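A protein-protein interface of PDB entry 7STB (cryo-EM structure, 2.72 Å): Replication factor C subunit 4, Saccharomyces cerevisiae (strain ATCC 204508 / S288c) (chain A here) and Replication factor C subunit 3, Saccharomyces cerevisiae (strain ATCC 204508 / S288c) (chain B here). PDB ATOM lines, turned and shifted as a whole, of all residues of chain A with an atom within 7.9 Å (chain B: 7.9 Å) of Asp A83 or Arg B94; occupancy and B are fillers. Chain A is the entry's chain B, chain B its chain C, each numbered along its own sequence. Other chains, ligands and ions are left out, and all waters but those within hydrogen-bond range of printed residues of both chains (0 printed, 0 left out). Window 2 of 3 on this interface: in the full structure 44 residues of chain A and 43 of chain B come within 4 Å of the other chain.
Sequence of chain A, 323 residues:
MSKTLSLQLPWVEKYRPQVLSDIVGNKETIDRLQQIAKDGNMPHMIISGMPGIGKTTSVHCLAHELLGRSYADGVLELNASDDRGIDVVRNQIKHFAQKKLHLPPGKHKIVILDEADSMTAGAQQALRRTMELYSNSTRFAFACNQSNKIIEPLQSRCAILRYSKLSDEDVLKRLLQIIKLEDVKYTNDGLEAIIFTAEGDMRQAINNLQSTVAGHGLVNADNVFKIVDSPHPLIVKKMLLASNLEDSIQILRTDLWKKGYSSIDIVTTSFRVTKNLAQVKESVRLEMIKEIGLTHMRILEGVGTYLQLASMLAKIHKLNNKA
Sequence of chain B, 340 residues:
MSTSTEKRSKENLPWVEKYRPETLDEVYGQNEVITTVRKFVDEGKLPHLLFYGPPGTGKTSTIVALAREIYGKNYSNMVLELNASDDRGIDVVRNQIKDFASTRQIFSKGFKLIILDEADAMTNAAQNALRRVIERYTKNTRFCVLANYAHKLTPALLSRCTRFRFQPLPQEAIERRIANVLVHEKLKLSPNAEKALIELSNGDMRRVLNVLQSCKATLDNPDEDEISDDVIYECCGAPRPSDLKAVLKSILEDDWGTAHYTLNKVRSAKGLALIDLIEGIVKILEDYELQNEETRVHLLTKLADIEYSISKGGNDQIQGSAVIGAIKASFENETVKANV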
ATOM      1  N   LEU A  78       6.975  -6.305 -28.553  1.00  0.00           N
ATOM      2  CA  LEU A  78       6.370  -7.313 -27.697  1.00  0.00           C
ATOM      3  C   LEU A  78       7.430  -7.889 -26.772  1.00  0.00           C
ATOM      4  O   LEU A  78       8.627  -7.872 -27.074  1.00  0.00           O
ATOM      5  CB  LEU A  78       5.715  -8.435 -28.517  1.00  0.00           C
ATOM      6  CG  LEU A  78       4.270  -8.194 -28.963  1.00  0.00           C
ATOM      7  CD1 LEU A  78       3.334  -8.127 -27.766  1.00  0.00           C
ATOM      8  CD2 LEU A  78       4.178  -6.921 -29.775  1.00  0.00           C
ATOM      9  N   ASN A  79       6.975  -8.402 -25.634  1.00  0.00           N
ATOM     10  CA  ASN A  79       7.876  -8.791 -24.559  1.00  0.00           C
ATOM     11  C   ASN A  79       7.176  -9.817 -23.680  1.00  0.00           C
ATOM     12  O   ASN A  79       5.978 -10.072 -23.819  1.00  0.00           O
ATOM     13  CB  ASN A  79       8.319  -7.559 -23.762  1.00  0.00           C
ATOM     14  CG  ASN A  79       7.162  -6.868 -23.062  1.00  0.00           C
ATOM     15  OD1 ASN A  79       6.037  -7.365 -23.057  1.00  0.00           O
ATOM     16  ND2 ASN A  79       7.427  -5.695 -22.500  1.00  0.00           N
ATOM     17  N   ALA A  80       7.950 -10.407 -22.766  1.00  0.00           N
ATOM     18  CA  ALA A  80       7.408 -11.451 -21.903  1.00  0.00           C
ATOM     19  C   ALA A  80       6.256 -10.925 -21.056  1.00  0.00           C
ATOM     20  O   ALA A  80       5.250 -11.618 -20.865  1.00  0.00           O
ATOM     21  CB  ALA A  80       8.511 -12.021 -21.014  1.00  0.00           C
ATOM     22  N   SER A  81       6.385  -9.703 -20.535  1.00  0.00           N
ATOM     23  CA  SER A  81       5.315  -9.128 -19.727  1.00  0.00           C
ATOM     24  C   SER A  81       4.024  -8.961 -20.516  1.00  0.00           C
ATOM     25  O   SER A  81       2.944  -8.948 -19.917  1.00  0.00           O
ATOM     26  CB  SER A  81       5.751  -7.777 -19.159  1.00  0.00           C
ATOM     27  OG  SER A  81       5.701  -6.766 -20.148  1.00  0.00           O
ATOM     28  N   ASP A  82       4.108  -8.828 -21.835  1.00  0.00           N
ATOM     29  CA  ASP A  82       2.936  -8.728 -22.688  1.00  0.00           C
ATOM     30  C   ASP A  82       2.537 -10.111 -23.183  1.00  0.00           C
ATOM     31  O   ASP A  82       3.384 -10.983 -23.395  1.00  0.00           O
ATOM     32  CB  ASP A  82       3.202  -7.807 -23.881  1.00  0.00           C
ATOM     33  CG  ASP A  82       3.357  -6.354 -23.476  1.00  0.00           C
ATOM     34  OD1 ASP A  82       2.752  -5.948 -22.462  1.00  0.00           O
ATOM     35  OD2 ASP A  82       4.084  -5.617 -24.174  1.00  0.00           O
ATOM     36  N   ASP A  83       1.233 -10.307 -23.361  1.00  0.00           N
ATOM     37  CA  ASP A  83       0.740 -11.578 -23.873  1.00  0.00           C
ATOM     38  C   ASP A  83       1.319 -11.841 -25.257  1.00  0.00           C
ATOM     39  O   ASP A  83       1.297 -10.968 -26.130  1.00  0.00           O
ATOM     40  CB  ASP A  83      -0.788 -11.568 -23.929  1.00  0.00           C
ATOM     41  CG  ASP A  83      -1.389 -12.956 -23.805  1.00  0.00           C
ATOM     42  OD1 ASP A  83      -0.661 -13.897 -23.424  1.00  0.00           O
ATOM     43  OD2 ASP A  83      -2.597 -13.107 -24.087  1.00  0.00           O
ATOM     44  N   ARG A  84       1.841 -13.050 -25.453  1.00  0.00           N
ATOM     45  CA  ARG A  84       2.482 -13.433 -26.707  1.00  0.00           C
ATOM     46  C   ARG A  84       2.050 -14.834 -27.114  1.00  0.00           C
ATOM     47  O   ARG A  84       2.870 -15.663 -27.521  1.00  0.00           O
ATOM     48  CB  ARG A  84       4.003 -13.350 -26.592  1.00  0.00           C
ATOM     49  CG  ARG A  84       4.537 -11.930 -26.516  1.00  0.00           C
ATOM     50  CD  ARG A  84       6.053 -11.902 -26.581  1.00  0.00           C
ATOM     51  NE  ARG A  84       6.659 -12.805 -25.610  1.00  0.00           N
ATOM     52  CZ  ARG A  84       7.965 -12.980 -25.465  1.00  0.00           C
ATOM     53  NH1 ARG A  84       8.839 -12.320 -26.208  1.00  0.00           N
ATOM     54  NH2 ARG A  84       8.406 -13.838 -24.549  1.00  0.00           N
ATOM     55  N   GLY A  85       0.755 -15.118 -27.006  1.00  0.00           N
ATOM     56  CA  GLY A  85       0.231 -16.417 -27.365  1.00  0.00           C
ATOM     57  C   GLY A  85      -0.018 -16.548 -28.854  1.00  0.00           C
ATOM     58  O   GLY A  85       0.272 -15.659 -29.654  1.00  0.00           O
ATOM     59  N   ILE A  86      -0.577 -17.700 -29.229  1.00  0.00           N
ATOM     60  CA  ILE A  86      -0.862 -17.957 -30.636  1.00  0.00           C
ATOM     61  C   ILE A  86      -1.908 -16.980 -31.154  1.00  0.00           C
ATOM     62  O   ILE A  86      -1.857 -16.551 -32.311  1.00  0.00           O
ATOM     63  CB  ILE A  86      -1.303 -19.420 -30.836  1.00  0.00           C
ATOM     64  CG1 ILE A  86      -1.374 -19.751 -32.329  1.00  0.00           C
ATOM     65  CG2 ILE A  86      -2.649 -19.674 -30.170  1.00  0.00           C
ATOM     66  CD1 ILE A  86      -1.317 -21.229 -32.626  1.00  0.00           C
ATOM     67  N   ASP A  87      -2.874 -16.613 -30.308  1.00  0.00           N
ATOM     68  CA  ASP A  87      -3.880 -15.637 -30.715  1.00  0.00           C
ATOM     69  C   ASP A  87      -3.251 -14.271 -30.963  1.00  0.00           C
ATOM     70  O   ASP A  87      -3.675 -13.537 -31.865  1.00  0.00           O
ATOM     71  CB  ASP A  87      -4.974 -15.542 -29.652  1.00  0.00           C
ATOM     72  CG  ASP A  87      -6.123 -14.650 -30.076  1.00  0.00           C
ATOM     73  OD1 ASP A  87      -6.925 -15.081 -30.930  1.00  0.00           O
ATOM     74  OD2 ASP A  87      -6.224 -13.520 -29.554  1.00  0.00           O
ATOM     75  N   VAL A  88      -2.246 -13.908 -30.164  1.00  0.00           N
ATOM     76  CA  VAL A  88      -1.550 -12.643 -30.377  1.00  0.00           C
ATOM     77  C   VAL A  88      -0.896 -12.630 -31.752  1.00  0.00           C
ATOM     78  O   VAL A  88      -1.030 -11.666 -32.514  1.00  0.00           O
ATOM     79  CB  VAL A  88      -0.519 -12.403 -29.260  1.00  0.00           C
ATOM     80  CG1 VAL A  88       0.317 -11.168 -29.562  1.00  0.00           C
ATOM     81  CG2 VAL A  88      -1.219 -12.267 -27.918  1.00  0.00           C
ATOM     82  N   VAL A  89      -0.196 -13.712 -32.100  1.00  0.00           N
ATOM     83  CA  VAL A  89       0.407 -13.810 -33.426  1.00  0.00           C
ATOM     84  C   VAL A  89      -0.672 -13.771 -34.498  1.00  0.00           C
ATOM     85  O   VAL A  89      -0.488 -13.179 -35.569  1.00  0.00           O
ATOM     86  CB  VAL A  89       1.260 -15.089 -33.531  1.00  0.00           C
ATOM     87  CG1 VAL A  89       1.924 -15.179 -34.899  1.00  0.00           C
ATOM     88  CG2 VAL A  89       2.302 -15.132 -32.423  1.00  0.00           C
ATOM     89  N   GLN A  92      -2.614  -9.529 -33.603  1.00  0.00           N
ATOM     90  CA  GLN A  92      -1.887  -8.266 -33.500  1.00  0.00           C
ATOM     91  C   GLN A  92      -0.691  -8.239 -34.443  1.00  0.00           C
ATOM     92  O   GLN A  92      -0.523  -7.294 -35.225  1.00  0.00           O
ATOM     93  CB  GLN A  92      -1.438  -8.038 -32.057  1.00  0.00           C
ATOM     94  CG  GLN A  92      -0.884  -6.646 -31.794  1.00  0.00           C
ATOM     95  CD  GLN A  92      -0.384  -6.474 -30.373  1.00  0.00           C
ATOM     96  OE1 GLN A  92      -0.151  -7.450 -29.662  1.00  0.00           O
ATOM     97  NE2 GLN A  92      -0.214  -5.226 -29.955  1.00  0.00           N
ATOM     98  N   ILE A  93       0.152  -9.272 -34.385  1.00  0.00           N
ATOM     99  CA  ILE A  93       1.304  -9.338 -35.278  1.00  0.00           C
ATOM    100  C   ILE A  93       0.842  -9.412 -36.726  1.00  0.00           C
ATOM    101  O   ILE A  93       1.428  -8.784 -37.614  1.00  0.00           O
ATOM    102  CB  ILE A  93       2.204 -10.532 -34.906  1.00  0.00           C
ATOM    103  CG1 ILE A  93       2.543 -10.494 -33.413  1.00  0.00           C
ATOM    104  CG2 ILE A  93       3.478 -10.525 -35.747  1.00  0.00           C
ATOM    105  CD1 ILE A  93       3.618 -11.474 -32.995  1.00  0.00           C
ATOM    106  N   LEU A 113      10.816  -8.746 -31.012  1.00  0.00           N
ATOM    107  CA  LEU A 113      10.344  -9.766 -30.079  1.00  0.00           C
ATOM    108  C   LEU A 113      11.429  -9.979 -29.026  1.00  0.00           C
ATOM    109  O   LEU A 113      12.185 -10.949 -29.055  1.00  0.00           O
ATOM    110  CB  LEU A 113      10.004 -11.056 -30.818  1.00  0.00           C
ATOM    111  CG  LEU A 113       8.763 -11.004 -31.712  1.00  0.00           C
ATOM    112  CD1 LEU A 113       8.667 -12.254 -32.570  1.00  0.00           C
ATOM    113  CD2 LEU A 113       7.506 -10.832 -30.879  1.00  0.00           C
ATOM    114  N   MET A 119       8.683 -17.681 -25.921  1.00  0.00           N
ATOM    115  CA  MET A 119       7.423 -17.792 -26.638  1.00  0.00           C
ATOM    116  C   MET A 119       6.996 -19.252 -26.758  1.00  0.00           C
ATOM    117  O   MET A 119       7.817 -20.171 -26.714  1.00  0.00           O
ATOM    118  CB  MET A 119       7.545 -17.171 -28.029  1.00  0.00           C
ATOM    119  CG  MET A 119       7.756 -15.670 -28.014  1.00  0.00           C
ATOM    120  SD  MET A 119       7.931 -14.976 -29.667  1.00  0.00           S
ATOM    121  CE  MET A 119       6.253 -15.140 -30.270  1.00  0.00           C
ATOM    122  N   THR A 120       5.690 -19.455 -26.906  1.00  0.00           N
ATOM    123  CA  THR A 120       5.142 -20.796 -27.025  1.00  0.00           C
ATOM    124  C   THR A 120       5.454 -21.387 -28.397  1.00  0.00           C
ATOM    125  O   THR A 120       5.704 -20.677 -29.373  1.00  0.00           O
ATOM    126  CB  THR A 120       3.630 -20.782 -26.798  1.00  0.00           C
ATOM    127  OG1 THR A 120       3.013 -19.858 -27.703  1.00  0.00           O
ATOM    128  CG2 THR A 120       3.308 -20.382 -25.367  1.00  0.00           C
ATOM    129  N   ARG B  88       1.075 -16.353  -7.581  1.00  0.00           N
ATOM    130  CA  ARG B  88       2.086 -15.523  -8.227  1.00  0.00           C
ATOM    131  C   ARG B  88       2.515 -16.144  -9.549  1.00  0.00           C
ATOM    132  O   ARG B  88       3.703 -16.258  -9.860  1.00  0.00           O
ATOM    133  CB  ARG B  88       3.285 -15.322  -7.306  1.00  0.00           C
ATOM    134  CG  ARG B  88       3.034 -14.335  -6.178  1.00  0.00           C
ATOM    135  CD  ARG B  88       4.298 -14.063  -5.381  1.00  0.00           C
ATOM    136  NE  ARG B  88       4.959 -15.292  -4.961  1.00  0.00           N
ATOM    137  CZ  ARG B  88       6.074 -15.336  -4.246  1.00  0.00           C
ATOM    138  NH1 ARG B  88       6.682 -14.232  -3.842  1.00  0.00           N
ATOM    139  NH2 ARG B  88       6.593 -16.518  -3.925  1.00  0.00           N
ATOM    140  N   GLY B  89       1.538 -16.559 -10.350  1.00  0.00           N
ATOM    141  CA  GLY B  89       1.813 -17.103 -11.660  1.00  0.00           C
ATOM    142  C   GLY B  89       2.091 -16.014 -12.677  1.00  0.00           C
ATOM    143  O   GLY B  89       2.092 -14.820 -12.381  1.00  0.00           O
ATOM    144  N   ILE B  90       2.334 -16.450 -13.914  1.00  0.00           N
ATOM    145  CA  ILE B  90       2.614 -15.500 -14.988  1.00  0.00           C
ATOM    146  C   ILE B  90       1.417 -14.585 -15.210  1.00  0.00           C
ATOM    147  O   ILE B  90       1.574 -13.396 -15.508  1.00  0.00           O
ATOM    148  CB  ILE B  90       3.005 -16.246 -16.277  1.00  0.00           C
ATOM    149  CG1 ILE B  90       3.647 -15.276 -17.272  1.00  0.00           C
ATOM    150  CG2 ILE B  90       1.791 -16.923 -16.898  1.00  0.00           C
ATOM    151  CD1 ILE B  90       3.986 -15.902 -18.606  1.00  0.00           C
ATOM    152  N   ASP B  91       0.203 -15.123 -15.080  1.00  0.00           N
ATOM    153  CA  ASP B  91      -0.995 -14.309 -15.266  1.00  0.00           C
ATOM    154  C   ASP B  91      -1.084 -13.212 -14.210  1.00  0.00           C
ATOM    155  O   ASP B  91      -1.418 -12.058 -14.520  1.00  0.00           O
ATOM    156  CB  ASP B  91      -2.232 -15.206 -15.221  1.00  0.00           C
ATOM    157  CG  ASP B  91      -3.500 -14.476 -15.613  1.00  0.00           C
ATOM    158  OD1 ASP B  91      -3.426 -13.262 -15.892  1.00  0.00           O
ATOM    159  OD2 ASP B  91      -4.570 -15.118 -15.644  1.00  0.00           O
ATOM    160  N   VAL B  92      -0.792 -13.553 -12.953  1.00  0.00           N
ATOM    161  CA  VAL B  92      -0.824 -12.558 -11.885  1.00  0.00           C
ATOM    162  C   VAL B  92       0.193 -11.459 -12.162  1.00  0.00           C
ATOM    163  O   VAL B  92      -0.114 -10.267 -12.067  1.00  0.00           O
ATOM    164  CB  VAL B  92      -0.572 -13.225 -10.521  1.00  0.00           C
ATOM    165  CG1 VAL B  92      -0.443 -12.172  -9.432  1.00  0.00           C
ATOM    166  CG2 VAL B  92      -1.687 -14.205 -10.194  1.00  0.00           C
ATOM    167  N   VAL B  93       1.415 -11.848 -12.527  1.00  0.00           N
ATOM    168  CA  VAL B  93       2.446 -10.864 -12.839  1.00  0.00           C
ATOM    169  C   VAL B  93       1.999  -9.980 -13.995  1.00  0.00           C
ATOM    170  O   VAL B  93       2.234  -8.765 -13.997  1.00  0.00           O
ATOM    171  CB  VAL B  93       3.779 -11.569 -13.152  1.00  0.00           C
ATOM    172  CG1 VAL B  93       4.763 -10.593 -13.779  1.00  0.00           C
ATOM    173  CG2 VAL B  93       4.362 -12.190 -11.894  1.00  0.00           C
ATOM    174  N   ARG B  94       1.349 -10.575 -14.995  1.00  0.00           N
ATOM    175  CA  ARG B  94       0.984  -9.835 -16.195  1.00  0.00           C
ATOM    176  C   ARG B  94      -0.180  -8.882 -15.970  1.00  0.00           C
ATOM    177  O   ARG B  94      -0.293  -7.891 -16.699  1.00  0.00           O
ATOM    178  CB  ARG B  94       0.642 -10.807 -17.325  1.00  0.00           C
ATOM    179  CG  ARG B  94       1.861 -11.365 -18.039  1.00  0.00           C
ATOM    180  CD  ARG B  94       1.494 -12.015 -19.361  1.00  0.00           C
ATOM    181  NE  ARG B  94       0.953 -13.359 -19.180  1.00  0.00           N
ATOM    182  CZ  ARG B  94      -0.256 -13.755 -19.558  1.00  0.00           C
ATOM    183  NH1 ARG B  94      -1.107 -12.932 -20.150  1.00  0.00           N
ATOM    184  NH2 ARG B  94      -0.623 -15.014 -19.337  1.00  0.00           N
ATOM    185  N   ASN B  95      -1.048  -9.146 -14.991  1.00  0.00           N
ATOM    186  CA  ASN B  95      -2.200  -8.278 -14.767  1.00  0.00           C
ATOM    187  C   ASN B  95      -2.094  -7.453 -13.489  1.00  0.00           C
ATOM    188  O   ASN B  95      -2.069  -6.222 -13.563  1.00  0.00           O
ATOM    189  CB  ASN B  95      -3.487  -9.116 -14.749  1.00  0.00           C
ATOM    190  CG  ASN B  95      -3.840  -9.670 -16.117  1.00  0.00           C
ATOM    191  OD1 ASN B  95      -4.115 -10.858 -16.265  1.00  0.00           O
ATOM    192  ND2 ASN B  95      -3.850  -8.802 -17.124  1.00  0.00           N
ATOM    193  N   GLN B  96      -1.983  -8.082 -12.318  1.00  0.00           N
ATOM    194  CA  GLN B  96      -2.077  -7.320 -11.075  1.00  0.00           C
ATOM    195  C   GLN B  96      -0.869  -6.407 -10.892  1.00  0.00           C
ATOM    196  O   GLN B  96      -1.017  -5.202 -10.646  1.00  0.00           O
ATOM    197  CB  GLN B  96      -2.216  -8.273  -9.887  1.00  0.00           C
ATOM    198  CG  GLN B  96      -2.281  -7.580  -8.535  1.00  0.00           C
ATOM    199  CD  GLN B  96      -2.370  -8.559  -7.382  1.00  0.00           C
ATOM    200  OE1 GLN B  96      -2.172  -9.761  -7.557  1.00  0.00           O
ATOM    201  NE2 GLN B  96      -2.671  -8.048  -6.195  1.00  0.00           N
ATOM    202  N   ILE B  97       0.336  -6.965 -11.014  1.00  0.00           N
ATOM    203  CA  ILE B  97       1.544  -6.174 -10.810  1.00  0.00           C
ATOM    204  C   ILE B  97       1.665  -5.107 -11.889  1.00  0.00           C
ATOM    205  O   ILE B  97       2.049  -3.965 -11.611  1.00  0.00           O
ATOM    206  CB  ILE B  97       2.782  -7.089 -10.771  1.00  0.00           C
ATOM    207  CG1 ILE B  97       2.573  -8.213  -9.750  1.00  0.00           C
ATOM    208  CG2 ILE B  97       4.031  -6.283 -10.432  1.00  0.00           C
ATOM    209  CD1 ILE B  97       3.789  -9.086  -9.532  1.00  0.00           C
ATOM    210  N   LYS B  98       1.346  -5.459 -13.135  1.00  0.00           N
ATOM    211  CA  LYS B  98       1.429  -4.483 -14.214  1.00  0.00           C
ATOM    212  C   LYS B  98       0.463  -3.328 -13.985  1.00  0.00           C
ATOM    213  O   LYS B  98       0.821  -2.162 -14.194  1.00  0.00           O
ATOM    214  CB  LYS B  98       1.153  -5.159 -15.557  1.00  0.00           C
ATOM    215  CG  LYS B  98       1.552  -4.320 -16.759  1.00  0.00           C
ATOM    216  CD  LYS B  98       1.678  -5.165 -18.015  1.00  0.00           C
ATOM    217  CE  LYS B  98       2.285  -4.370 -19.158  1.00  0.00           C
ATOM    218  NZ  LYS B  98       2.415  -5.181 -20.400  1.00  0.00           N
ATOM    219  N   ASP B  99      -0.766  -3.626 -13.552  1.00  0.00           N
ATOM    220  CA  ASP B  99      -1.721  -2.560 -13.274  1.00  0.00           C
ATOM    221  C   ASP B  99      -1.251  -1.689 -12.117  1.00  0.00           C
ATOM    222  O   ASP B  99      -1.371  -0.461 -12.169  1.00  0.00           O
ATOM    223  CB  ASP B  99      -3.096  -3.156 -12.969  1.00  0.00           C
ATOM    224  CG  ASP B  99      -3.681  -3.906 -14.149  1.00  0.00           C
ATOM    225  OD1 ASP B  99      -3.151  -3.761 -15.271  1.00  0.00           O
ATOM    226  OD2 ASP B  99      -4.670  -4.643 -13.954  1.00  0.00           O
ATOM    227  N   ALA B 125       8.745 -18.579 -15.777  1.00  0.00           N
ATOM    228  CA  ALA B 125       7.979 -17.732 -16.685  1.00  0.00           C
ATOM    229  C   ALA B 125       7.546 -16.444 -15.998  1.00  0.00           C
ATOM    230  O   ALA B 125       7.581 -15.364 -16.602  1.00  0.00           O
ATOM    231  CB  ALA B 125       6.763 -18.494 -17.212  1.00  0.00           C
ATOM    232  N   ALA B 126       7.130 -16.538 -14.734  1.00  0.00           N
ATOM    233  CA  ALA B 126       6.735 -15.344 -13.997  1.00  0.00           C
ATOM    234  C   ALA B 126       7.902 -14.376 -13.854  1.00  0.00           C
ATOM    235  O   ALA B 126       7.737 -13.167 -14.038  1.00  0.00           O
ATOM    236  CB  ALA B 126       6.189 -15.733 -12.624  1.00  0.00           C
ATOM    237  N   ALA B 129       8.583 -12.681 -17.215  1.00  0.00           N
ATOM    238  CA  ALA B 129       7.615 -11.621 -17.475  1.00  0.00           C
ATOM    239  C   ALA B 129       7.861 -10.414 -16.578  1.00  0.00           C
ATOM    240  O   ALA B 129       7.688  -9.268 -17.007  1.00  0.00           O
ATOM    241  CB  ALA B 129       6.195 -12.151 -17.284  1.00  0.00           C
ATOM    242  N   LEU B 130       8.267 -10.651 -15.329  1.00  0.00           N
ATOM    243  CA  LEU B 130       8.438  -9.567 -14.370  1.00  0.00           C
ATOM    244  C   LEU B 130       9.688  -8.740 -14.631  1.00  0.00           C
ATOM    245  O   LEU B 130       9.741  -7.578 -14.218  1.00  0.00           O
ATOM    246  CB  LEU B 130       8.488 -10.139 -12.952  1.00  0.00           C
ATOM    247  CG  LEU B 130       8.358  -9.153 -11.789  1.00  0.00           C
ATOM    248  CD1 LEU B 130       7.096  -8.310 -11.905  1.00  0.00           C
ATOM    249  CD2 LEU B 130       8.382  -9.908 -10.470  1.00  0.00           C
ATOM    250  N   VAL B 133       8.711  -5.850 -16.769  1.00  0.00           N
ATOM    251  CA  VAL B 133       7.871  -4.951 -15.980  1.00  0.00           C
ATOM    252  C   VAL B 133       8.740  -4.090 -15.076  1.00  0.00           C
ATOM    253  O   VAL B 133       8.520  -2.880 -14.940  1.00  0.00           O
ATOM    254  CB  VAL B 133       6.838  -5.755 -15.169  1.00  0.00           C
ATOM    255  CG1 VAL B 133       6.074  -4.841 -14.217  1.00  0.00           C
ATOM    256  CG2 VAL B 133       5.885  -6.484 -16.094  1.00  0.00           C
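The side-chain carboxylate of Asp A83 is in salt-bridge range of the guanidinium group of Arg B94, at 3.4 Å.
The side-chain carboxylate (OD1) of Asp A82 sits close to the side-chain amino group (NZ) of Lys B98 (2.2 Å).
The side-chain amide oxygen (OD1) of Asn A79 sits at hydrogen-bond distance from the side-chain hydroxyl (OG) of Ser A81.
OD1 of Asn A79 is in hydrogen-bond range of N of Asp A82, at 2.7 Å.
Among the printed residues, merely in contact across the chains: Ala A80 with Ala B129, Ser A81 with Arg B94, Ser A81 with Lys B98, Ser A81 with Ala B129 and Ser A81 with Val B133.
Printed residues of chain B within 4 Å of Asp A82: Lys B98.
Asp A83 touches one residue of chain B.
Arg B88 touches none of the printed residues of chain A.
Val B93 touches none of the printed residues of chain A.
Arg B94 touches just these residues of chain A: Ser A81 (3.2 Å) and Asp A83 (3.4 Å).
Of the printed residues of chain A, Val B133 touches Ser A81 (3.3 Å).
The nearest residue of chain B that does not touch Asp A83 is Lys B98 (6.0 Å).
The nearest residue of chain A that does not touch Arg B94 is Ala A80 (4.1 Å).
Printed residues of chain B that touch a printed residue of chain A: Arg B94, Lys B98, Ala B129 and Val B133.
Hydrophobic or aromatic side chains of chain B within 4 Å of the printed part of chain A: Ala B129 and Val B133.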
